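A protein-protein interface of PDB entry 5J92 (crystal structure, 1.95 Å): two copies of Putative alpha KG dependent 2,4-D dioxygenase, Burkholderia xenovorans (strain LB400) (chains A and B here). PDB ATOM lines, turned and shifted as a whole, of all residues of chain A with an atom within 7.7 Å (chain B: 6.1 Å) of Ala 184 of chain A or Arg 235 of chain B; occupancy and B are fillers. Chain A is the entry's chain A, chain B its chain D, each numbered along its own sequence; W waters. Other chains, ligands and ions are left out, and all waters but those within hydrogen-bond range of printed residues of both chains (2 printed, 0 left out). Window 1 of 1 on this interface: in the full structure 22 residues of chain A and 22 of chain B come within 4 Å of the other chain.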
ATOM      1  N   LEU A 116       1.372  36.180  17.148  1.00  0.00           N
ATOM      2  CA  LEU A 116       0.929  34.800  16.976  1.00  0.00           C
ATOM      3  C   LEU A 116       1.329  33.912  18.152  1.00  0.00           C
ATOM      4  O   LEU A 116       0.546  33.056  18.572  1.00  0.00           O
ATOM      5  CB  LEU A 116       1.480  34.235  15.669  1.00  0.00           C
ATOM      6  CG  LEU A 116       0.909  34.871  14.402  1.00  0.00           C
ATOM      7  CD1 LEU A 116       1.513  34.254  13.151  1.00  0.00           C
ATOM      8  CD2 LEU A 116      -0.616  34.750  14.393  1.00  0.00           C
ATOM      9  N   THR A 117       2.549  34.058  18.674  1.00  0.00           N
ATOM     10  CA  THR A 117       2.935  33.208  19.796  1.00  0.00           C
ATOM     11  C   THR A 117       2.153  33.552  21.054  1.00  0.00           C
ATOM     12  O   THR A 117       1.932  32.675  21.899  1.00  0.00           O
ATOM     13  CB  THR A 117       4.434  33.310  20.063  1.00  0.00           C
ATOM     14  OG1 THR A 117       4.758  34.650  20.454  1.00  0.00           O
ATOM     15  CG2 THR A 117       5.201  32.948  18.799  1.00  0.00           C
ATOM     16  N   ARG A 120      -0.977  31.495  22.140  1.00  0.00           N
ATOM     17  CA  ARG A 120      -0.792  30.240  22.850  1.00  0.00           C
ATOM     18  C   ARG A 120      -0.605  30.518  24.339  1.00  0.00           C
ATOM     19  O   ARG A 120       0.058  31.491  24.722  1.00  0.00           O
ATOM     20  CB  ARG A 120       0.412  29.480  22.266  1.00  0.00           C
ATOM     21  CG  ARG A 120       0.147  28.973  20.827  1.00  0.00           C
ATOM     22  CD  ARG A 120       1.366  29.004  19.923  1.00  0.00           C
ATOM     23  NE  ARG A 120       1.088  28.440  18.596  1.00  0.00           N
ATOM     24  CZ  ARG A 120       0.686  29.143  17.534  1.00  0.00           C
ATOM     25  NH1 ARG A 120       0.502  30.452  17.626  1.00  0.00           N
ATOM     26  NH2 ARG A 120       0.476  28.544  16.368  1.00  0.00           N
ATOM     27  N   ILE A 178      12.597  28.934  24.636  1.00  0.00           N
ATOM     28  CA  ILE A 178      11.847  29.855  23.783  1.00  0.00           C
ATOM     29  C   ILE A 178      11.990  29.479  22.311  1.00  0.00           C
ATOM     30  O   ILE A 178      11.030  29.581  21.538  1.00  0.00           O
ATOM     31  CB  ILE A 178      12.277  31.314  24.051  1.00  0.00           C
ATOM     32  CG1 ILE A 178      11.396  32.301  23.277  1.00  0.00           C
ATOM     33  CG2 ILE A 178      13.759  31.538  23.735  1.00  0.00           C
ATOM     34  CD1 ILE A 178       9.932  32.244  23.635  1.00  0.00           C
ATOM     35  N   MET A 179      13.173  29.016  21.903  1.00  0.00           N
ATOM     36  CA  MET A 179      13.381  28.681  20.498  1.00  0.00           C
ATOM     37  C   MET A 179      12.558  27.465  20.107  1.00  0.00           C
ATOM     38  O   MET A 179      12.025  27.398  18.995  1.00  0.00           O
ATOM     39  CB  MET A 179      14.873  28.451  20.224  1.00  0.00           C
ATOM     40  CG  MET A 179      15.729  29.696  20.386  1.00  0.00           C
ATOM     41  SD  MET A 179      15.100  31.079  19.408  1.00  0.00           S
ATOM     42  CE  MET A 179      15.953  32.476  20.160  1.00  0.00           C
ATOM     43  N   ALA A 180      12.410  26.507  21.020  1.00  0.00           N
ATOM     44  CA  ALA A 180      11.540  25.369  20.747  1.00  0.00           C
ATOM     45  C   ALA A 180      10.078  25.800  20.628  1.00  0.00           C
ATOM     46  O   ALA A 180       9.359  25.327  19.737  1.00  0.00           O
ATOM     47  CB  ALA A 180      11.706  24.309  21.833  1.00  0.00           C
ATOM     48  N   SER A 181       9.614  26.702  21.505  1.00  0.00           N
ATOM     49  CA  SER A 181       8.215  27.123  21.424  1.00  0.00           C
ATOM     50  C   SER A 181       7.963  27.961  20.178  1.00  0.00           C
ATOM     51  O   SER A 181       6.895  27.855  19.558  1.00  0.00           O
ATOM     52  CB  SER A 181       7.800  27.898  22.681  1.00  0.00           C
ATOM     53  OG  SER A 181       8.446  29.170  22.750  1.00  0.00           O
ATOM     54  N   ARG A 182       8.926  28.798  19.794  1.00  0.00           N
ATOM     55  CA  ARG A 182       8.793  29.535  18.544  1.00  0.00           C
ATOM     56  C   ARG A 182       8.749  28.589  17.358  1.00  0.00           C
ATOM     57  O   ARG A 182       7.941  28.776  16.438  1.00  0.00           O
ATOM     58  CB  ARG A 182       9.944  30.530  18.394  1.00  0.00           C
ATOM     59  CG  ARG A 182       9.836  31.757  19.278  1.00  0.00           C
ATOM     60  CD  ARG A 182      11.033  32.641  19.051  1.00  0.00           C
ATOM     61  NE  ARG A 182      11.087  33.772  19.970  1.00  0.00           N
ATOM     62  CZ  ARG A 182      12.115  34.614  20.018  1.00  0.00           C
ATOM     63  NH1 ARG A 182      13.152  34.431  19.207  1.00  0.00           N
ATOM     64  NH2 ARG A 182      12.110  35.630  20.873  1.00  0.00           N
ATOM     65  N   ALA A 183       9.611  27.565  17.357  1.00  0.00           N
ATOM     66  CA  ALA A 183       9.602  26.600  16.261  1.00  0.00           C
ATOM     67  C   ALA A 183       8.267  25.864  16.182  1.00  0.00           C
ATOM     68  O   ALA A 183       7.759  25.611  15.083  1.00  0.00           O
ATOM     69  CB  ALA A 183      10.757  25.615  16.421  1.00  0.00           C
ATOM     70  N   ALA A 184       7.671  25.537  17.336  1.00  0.00           N
ATOM     71  CA  ALA A 184       6.352  24.907  17.339  1.00  0.00           C
ATOM     72  C   ALA A 184       5.291  25.826  16.752  1.00  0.00           C
ATOM     73  O   ALA A 184       4.287  25.346  16.209  1.00  0.00           O
ATOM     74  CB  ALA A 184       5.952  24.499  18.761  1.00  0.00           C
ATOM     75  N   ALA A 185       5.483  27.140  16.858  1.00  0.00           N
ATOM     76  CA  ALA A 185       4.580  28.094  16.225  1.00  0.00           C
ATOM     77  C   ALA A 185       4.967  28.405  14.786  1.00  0.00           C
ATOM     78  O   ALA A 185       4.319  29.245  14.148  1.00  0.00           O
ATOM     79  CB  ALA A 185       4.522  29.388  17.036  1.00  0.00           C
ATOM     80  N   GLY A 186       6.013  27.766  14.267  1.00  0.00           N
ATOM     81  CA  GLY A 186       6.421  27.950  12.886  1.00  0.00           C
ATOM     82  C   GLY A 186       7.509  28.976  12.649  1.00  0.00           C
ATOM     83  O   GLY A 186       7.714  29.371  11.493  1.00  0.00           O
ATOM     84  N   PHE A 187       8.200  29.429  13.695  1.00  0.00           N
ATOM     85  CA  PHE A 187       9.263  30.419  13.582  1.00  0.00           C
ATOM     86  C   PHE A 187      10.597  29.737  13.839  1.00  0.00           C
ATOM     87  O   PHE A 187      10.827  29.215  14.933  1.00  0.00           O
ATOM     88  CB  PHE A 187       9.065  31.574  14.567  1.00  0.00           C
ATOM     89  CG  PHE A 187       7.839  32.403  14.299  1.00  0.00           C
ATOM     90  CD1 PHE A 187       7.881  33.451  13.394  1.00  0.00           C
ATOM     91  CD2 PHE A 187       6.658  32.158  14.978  1.00  0.00           C
ATOM     92  CE1 PHE A 187       6.754  34.219  13.147  1.00  0.00           C
ATOM     93  CE2 PHE A 187       5.533  32.931  14.742  1.00  0.00           C
ATOM     94  CZ  PHE A 187       5.580  33.951  13.826  1.00  0.00           C
ATOM     95  N   TYR A 188      11.475  29.753  12.840  1.00  0.00           N
ATOM     96  CA  TYR A 188      12.741  29.047  12.924  1.00  0.00           C
ATOM     97  C   TYR A 188      13.938  29.966  12.760  1.00  0.00           C
ATOM     98  O   TYR A 188      15.072  29.515  12.948  1.00  0.00           O
ATOM     99  CB  TYR A 188      12.807  27.947  11.856  1.00  0.00           C
ATOM    100  CG  TYR A 188      11.597  27.049  11.831  1.00  0.00           C
ATOM    101  CD1 TYR A 188      11.510  25.956  12.686  1.00  0.00           C
ATOM    102  CD2 TYR A 188      10.535  27.292  10.958  1.00  0.00           C
ATOM    103  CE1 TYR A 188      10.403  25.123  12.677  1.00  0.00           C
ATOM    104  CE2 TYR A 188       9.417  26.464  10.941  1.00  0.00           C
ATOM    105  CZ  TYR A 188       9.361  25.381  11.808  1.00  0.00           C
ATOM    106  OH  TYR A 188       8.273  24.540  11.811  1.00  0.00           O
ATOM    107  N   SER A 221       3.598  27.519  27.344  1.00  0.00           N
ATOM    108  CA  SER A 221       3.987  27.017  26.032  1.00  0.00           C
ATOM    109  C   SER A 221       5.502  26.885  25.912  1.00  0.00           C
ATOM    110  O   SER A 221       5.982  26.159  25.036  1.00  0.00           O
ATOM    111  CB  SER A 221       3.468  27.940  24.933  1.00  0.00           C
ATOM    112  OG  SER A 221       4.129  29.193  25.013  1.00  0.00           O
ATOM    113  N   ARG A 235       6.605  15.295  27.375  1.00  0.00           N
ATOM    114  CA  ARG A 235       5.683  16.034  26.515  1.00  0.00           C
ATOM    115  C   ARG A 235       4.239  15.611  26.753  1.00  0.00           C
ATOM    116  O   ARG A 235       3.328  16.449  26.779  1.00  0.00           O
ATOM    117  CB  ARG A 235       6.057  15.808  25.051  1.00  0.00           C
ATOM    118  CG  ARG A 235       7.393  16.426  24.697  1.00  0.00           C
ATOM    119  CD  ARG A 235       7.560  16.524  23.212  1.00  0.00           C
ATOM    120  NE  ARG A 235       8.761  17.272  22.884  1.00  0.00           N
ATOM    121  CZ  ARG A 235       8.764  18.579  22.645  1.00  0.00           C
ATOM    122  NH1 ARG A 235       7.634  19.264  22.706  1.00  0.00           N
ATOM    123  NH2 ARG A 235       9.900  19.194  22.344  1.00  0.00           N
ATOM    124  N   ALA B 180       6.634  14.659  11.250  1.00  0.00           N
ATOM    125  CA  ALA B 180       6.529  15.892  12.023  1.00  0.00           C
ATOM    126  C   ALA B 180       5.650  15.700  13.259  1.00  0.00           C
ATOM    127  O   ALA B 180       5.989  16.181  14.348  1.00  0.00           O
ATOM    128  CB  ALA B 180       5.998  17.020  11.143  1.00  0.00           C
ATOM    129  N   ALA B 223      -1.758  16.890  10.621  1.00  0.00           N
ATOM    130  CA  ALA B 223      -1.712  18.098   9.804  1.00  0.00           C
ATOM    131  C   ALA B 223      -0.795  19.136  10.442  1.00  0.00           C
ATOM    132  O   ALA B 223      -0.954  19.475  11.614  1.00  0.00           O
ATOM    133  CB  ALA B 223      -3.112  18.679   9.615  1.00  0.00           C
ATOM    134  N   THR B 224       0.141  19.666   9.665  1.00  0.00           N
ATOM    135  CA  THR B 224       1.112  20.609  10.202  1.00  0.00           C
ATOM    136  C   THR B 224       0.773  22.061   9.884  1.00  0.00           C
ATOM    137  O   THR B 224       0.779  22.904  10.787  1.00  0.00           O
ATOM    138  CB  THR B 224       2.514  20.259   9.688  1.00  0.00           C
ATOM    139  OG1 THR B 224       2.536  20.260   8.247  1.00  0.00           O
ATOM    140  CG2 THR B 224       2.917  18.892  10.204  1.00  0.00           C
ATOM    141  N   HIS B 225       0.490  22.385   8.628  1.00  0.00           N
ATOM    142  CA  HIS B 225       0.214  23.773   8.266  1.00  0.00           C
ATOM    143  C   HIS B 225      -0.518  23.810   6.927  1.00  0.00           C
ATOM    144  O   HIS B 225      -0.847  22.773   6.346  1.00  0.00           O
ATOM    145  CB  HIS B 225       1.506  24.614   8.253  1.00  0.00           C
ATOM    146  CG  HIS B 225       2.559  24.137   7.298  1.00  0.00           C
ATOM    147  ND1 HIS B 225       3.156  22.899   7.398  1.00  0.00           N
ATOM    148  CD2 HIS B 225       3.162  24.761   6.255  1.00  0.00           C
ATOM    149  CE1 HIS B 225       4.068  22.770   6.449  1.00  0.00           C
ATOM    150  NE2 HIS B 225       4.093  23.887   5.742  1.00  0.00           N
ATOM    151  N   VAL B 226      -0.773  25.024   6.440  1.00  0.00           N
ATOM    152  CA  VAL B 226      -1.653  25.250   5.297  1.00  0.00           C
ATOM    153  C   VAL B 226      -0.792  25.427   4.052  1.00  0.00           C
ATOM    154  O   VAL B 226       0.160  26.210   4.062  1.00  0.00           O
ATOM    155  CB  VAL B 226      -2.559  26.472   5.537  1.00  0.00           C
ATOM    156  CG1 VAL B 226      -3.369  26.830   4.288  1.00  0.00           C
ATOM    157  CG2 VAL B 226      -3.511  26.203   6.725  1.00  0.00           C
ATOM    158  N   PRO B 230       2.417  31.048   4.675  1.00  0.00           N
ATOM    159  CA  PRO B 230       3.560  31.000   5.595  1.00  0.00           C
ATOM    160  C   PRO B 230       3.222  30.091   6.767  1.00  0.00           C
ATOM    161  O   PRO B 230       2.063  29.995   7.182  1.00  0.00           O
ATOM    162  CB  PRO B 230       3.735  32.456   6.033  1.00  0.00           C
ATOM    163  CG  PRO B 230       3.016  33.263   4.989  1.00  0.00           C
ATOM    164  CD  PRO B 230       1.873  32.405   4.525  1.00  0.00           C
ATOM    165  N   GLU B 231       4.229  29.373   7.264  1.00  0.00           N
ATOM    166  CA  GLU B 231       3.980  28.385   8.314  1.00  0.00           C
ATOM    167  C   GLU B 231       3.281  28.971   9.534  1.00  0.00           C
ATOM    168  O   GLU B 231       2.305  28.371  10.008  1.00  0.00           O
ATOM    169  CB  GLU B 231       5.295  27.708   8.737  1.00  0.00           C
ATOM    170  CG  GLU B 231       5.899  26.781   7.706  1.00  0.00           C
ATOM    171  CD  GLU B 231       6.672  25.628   8.337  1.00  0.00           C
ATOM    172  OE1 GLU B 231       6.458  25.329   9.532  1.00  0.00           O
ATOM    173  OE2 GLU B 231       7.493  25.010   7.635  1.00  0.00           O
ATOM    174  N   PRO B 232       3.719  30.109  10.094  1.00  0.00           N
ATOM    175  CA  PRO B 232       3.066  30.575  11.333  1.00  0.00           C
ATOM    176  C   PRO B 232       1.575  30.843  11.175  1.00  0.00           C
ATOM    177  O   PRO B 232       0.790  30.442  12.042  1.00  0.00           O
ATOM    178  CB  PRO B 232       3.847  31.850  11.673  1.00  0.00           C
ATOM    179  CG  PRO B 232       5.169  31.656  11.045  1.00  0.00           C
ATOM    180  CD  PRO B 232       4.875  30.958   9.750  1.00  0.00           C
ATOM    181  N   GLU B 233       1.157  31.510  10.094  1.00  0.00           N
ATOM    182  CA  GLU B 233      -0.270  31.764   9.904  1.00  0.00           C
ATOM    183  C   GLU B 233      -1.039  30.463   9.719  1.00  0.00           C
ATOM    184  O   GLU B 233      -2.162  30.320  10.220  1.00  0.00           O
ATOM    185  CB  GLU B 233      -0.489  32.694   8.705  1.00  0.00           C
ATOM    186  CG  GLU B 233      -0.206  34.157   9.004  1.00  0.00           C
ATOM    187  CD  GLU B 233       1.271  34.489   9.114  1.00  0.00           C
ATOM    188  OE1 GLU B 233       2.127  33.638   8.755  1.00  0.00           O
ATOM    189  OE2 GLU B 233       1.578  35.621   9.564  1.00  0.00           O
ATOM    190  N   GLY B 234      -0.441  29.492   9.025  1.00  0.00           N
ATOM    191  CA  GLY B 234      -1.098  28.205   8.857  1.00  0.00           C
ATOM    192  C   GLY B 234      -1.199  27.432  10.158  1.00  0.00           C
ATOM    193  O   GLY B 234      -2.254  26.872  10.481  1.00  0.00           O
ATOM    194  N   ARG B 235      -0.113  27.408  10.935  1.00  0.00           N
ATOM    195  CA  ARG B 235      -0.161  26.728  12.223  1.00  0.00           C
ATOM    196  C   ARG B 235      -1.195  27.364  13.132  1.00  0.00           C
ATOM    197  O   ARG B 235      -1.890  26.662  13.879  1.00  0.00           O
ATOM    198  CB  ARG B 235       1.208  26.750  12.900  1.00  0.00           C
ATOM    199  CG  ARG B 235       2.236  25.921  12.193  1.00  0.00           C
ATOM    200  CD  ARG B 235       3.442  25.645  13.067  1.00  0.00           C
ATOM    201  NE  ARG B 235       4.327  24.720  12.379  1.00  0.00           N
ATOM    202  CZ  ARG B 235       4.346  23.405  12.566  1.00  0.00           C
ATOM    203  NH1 ARG B 235       3.532  22.828  13.444  1.00  0.00           N
ATOM    204  NH2 ARG B 235       5.194  22.670  11.859  1.00  0.00           N
ATOM    205  N   ASP B 236      -1.309  28.694  13.089  1.00  0.00           N
ATOM    206  CA  ASP B 236      -2.243  29.356  13.988  1.00  0.00           C
ATOM    207  C   ASP B 236      -3.691  29.066  13.615  1.00  0.00           C
ATOM    208  O   ASP B 236      -4.545  28.924  14.501  1.00  0.00           O
ATOM    209  CB  ASP B 236      -2.000  30.856  14.009  1.00  0.00           C
ATOM    210  CG  ASP B 236      -2.753  31.524  15.130  1.00  0.00           C
ATOM    211  OD1 ASP B 236      -2.376  31.305  16.305  1.00  0.00           O
ATOM    212  OD2 ASP B 236      -3.727  32.246  14.834  1.00  0.00           O
ATOM    213  N   LEU B 237      -3.993  28.992  12.318  1.00  0.00           N
ATOM    214  CA  LEU B 237      -5.347  28.638  11.896  1.00  0.00           C
ATOM    215  C   LEU B 237      -5.710  27.232  12.353  1.00  0.00           C
ATOM    216  O   LEU B 237      -6.805  27.003  12.882  1.00  0.00           O
ATOM    217  CB  LEU B 237      -5.487  28.740  10.378  1.00  0.00           C
ATOM    218  CG  LEU B 237      -6.847  28.272   9.835  1.00  0.00           C
ATOM    219  CD1 LEU B 237      -7.986  29.203  10.285  1.00  0.00           C
ATOM    220  CD2 LEU B 237      -6.821  28.146   8.319  1.00  0.00           C
ATOM    221  N   LEU B 238      -4.797  26.277  12.166  1.00  0.00           N
ATOM    222  CA  LEU B 238      -5.090  24.908  12.577  1.00  0.00           C
ATOM    223  C   LEU B 238      -5.250  24.804  14.087  1.00  0.00           C
ATOM    224  O   LEU B 238      -6.058  23.996  14.566  1.00  0.00           O
ATOM    225  CB  LEU B 238      -4.003  23.961  12.070  1.00  0.00           C
ATOM    226  CG  LEU B 238      -3.971  23.825  10.541  1.00  0.00           C
ATOM    227  CD1 LEU B 238      -2.915  22.820  10.131  1.00  0.00           C
ATOM    228  CD2 LEU B 238      -5.347  23.413  10.013  1.00  0.00           C
ATOM    229  N   ARG B 239      -4.481  25.602  14.841  1.00  0.00           N
ATOM    230  CA  ARG B 239      -4.627  25.661  16.292  1.00  0.00           C
ATOM    231  C   ARG B 239      -6.016  26.145  16.689  1.00  0.00           C
ATOM    232  O   ARG B 239      -6.674  25.550  17.553  1.00  0.00           O
ATOM    233  CB  ARG B 239      -3.554  26.585  16.889  1.00  0.00           C
ATOM    234  CG  ARG B 239      -3.701  26.779  18.403  1.00  0.00           C
ATOM    235  CD  ARG B 239      -3.051  28.078  18.915  1.00  0.00           C
ATOM    236  NE  ARG B 239      -3.525  29.274  18.216  1.00  0.00           N
ATOM    237  CZ  ARG B 239      -4.723  29.821  18.393  1.00  0.00           C
ATOM    238  NH1 ARG B 239      -5.588  29.273  19.250  1.00  0.00           N
ATOM    239  NH2 ARG B 239      -5.063  30.908  17.705  1.00  0.00           N
ATOM    240  N   GLU B 240      -6.465  27.241  16.074  1.00  0.00           N
ATOM    241  CA  GLU B 240      -7.782  27.791  16.373  1.00  0.00           C
ATOM    242  C   GLU B 240      -8.884  26.812  15.992  1.00  0.00           C
ATOM    243  O   GLU B 240      -9.801  26.563  16.782  1.00  0.00           O
ATOM    244  CB  GLU B 240      -7.954  29.127  15.643  1.00  0.00           C
ATOM    245  CG  GLU B 240      -9.255  29.881  15.926  1.00  0.00           C
ATOM    246  CD  GLU B 240      -9.264  30.578  17.284  1.00  0.00           C
ATOM    247  OE1 GLU B 240      -8.198  30.633  17.945  1.00  0.00           O
ATOM    248  OE2 GLU B 240     -10.341  31.065  17.695  1.00  0.00           O
HETATM  249  O   HOH W   1       1.325  24.179  15.048  1.00  0.00           O
HETATM  250  O   HOH W   2       1.818  30.266  14.615  1.00  0.00           O
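Water W2 lies within hydrogen-bond range of the backbone carbonyl oxygen of Ala 185 of chain A (2.7 Å), the backbone carbonyl oxygen of Pro 232 of chain B (2.8 Å) and the guanidinium group of Arg 120 of chain A (2.8 Å).
Water W1 lies within hydrogen-bond range of NH1 of Arg 235 of chain B (3.0 Å) and O of Ala 184 of chain A (3.4 Å).
Ala 184 of chain A touches one residue of chain B.
Printed residues of chain A within 4 Å of Arg 235 of chain B: Arg 120 (3.8 Å), Ala 184 (3.3 Å), Ala 185 (3.6 Å), Gly 186 (3.5 Å) and Tyr 188 (3.6 Å).
Gly 234 of chain B touches none of the printed residues of chain A.
Of the printed residues of chain A, Glu 231 of chain B touches Tyr 188.
Printed residues of chain B within 4 Å of Ala 185 of chain A: Pro 232 and Arg 235.
Printed residues of chain B within 4 Å of Gly 186 of chain A: Pro 232 and Arg 235.
Ala 223 of chain B touches none of the printed residues of chain A.
Ala 183 of chain A touches none of the printed residues of chain B.
Among the printed residues, merely in contact across the chains: Leu 116 of chain A with Pro 232 of chain B (3.7 Å), Leu 116 of chain A with Glu 233 of chain B (3.8 Å), Leu 116 of chain A with Asp 236 of chain B (3.9 Å), Arg 120 of chain A with Arg 235 of chain B (3.8 Å), Arg 120 of chain A with Arg 239 of chain B (3.8 Å), Ala 184 of chain A with Arg 235 of chain B (3.3 Å), Ala 185 of chain A with Pro 232 of chain B (3.4 Å), Ala 185 of chain A with Arg 235 of chain B (3.6 Å), Gly 186 of chain A with Pro 232 of chain B (3.4 Å), Gly 186 of chain A with Arg 235 of chain B (3.5 Å), Phe 187 of chain A with Pro 232 of chain B (3.5 Å) and Tyr 188 of chain A with Arg 235 of chain B (3.6 Å).
The backbone carbonyl oxygen (O) of Leu 116 of chain A sits at hydrogen-bond distance from the guanidinium group (NH1) of Arg 120 of chain A.
N of Phe 187 of chain A is in hydrogen-bond range of O of Arg 182 of chain A.
The backbone carbonyl oxygen of Ala 183 of chain A sits at hydrogen-bond distance from the side-chain hydroxyl of Tyr 188 of chain A (3.5 Å).
The side-chain carboxylate of Glu 231 of chain B lies within salt-bridge range of the guanidinium group of Arg 235 of chain B.
The guanidinium group (NE) of Arg 239 of chain B lies within salt-bridge range of the side-chain carboxylate (OD1) of Asp 236 of chain B, 3.0 Å away.
NH2 of Arg 239 of chain B lies within salt-bridge range of OE1 of Glu 240 of chain B.
The side-chain carboxylate (OD1) of Asp 236 of chain B lies within salt-bridge range of the guanidinium group (NH1) of Arg 120 of chain A (3.3 Å).
OH of Tyr 188 of chain A lies within hydrogen-bond range of OE1 of Glu 231 of chain B.
Positions printed for both chains: 180 and 235.
Of the 14 pairs that touch across the chains among the printed residues, none has its exchanged pair printed and touching as well.
Of the 16 printed residues of chain B, 6 touch a printed residue of chain A.
Hydrophobic or aromatic side chains of chain B within 4 Å of the printed part of chain A: Pro 232.
Among the printed residues, 14 pairs touch across the chains.
Among the printed residues, Asp or Glu carboxylates within 4 Å of a Lys or Arg side-chain nitrogen of the other chain: Arg 120 of chain A with Asp 236 of chain B (3.3 Å).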
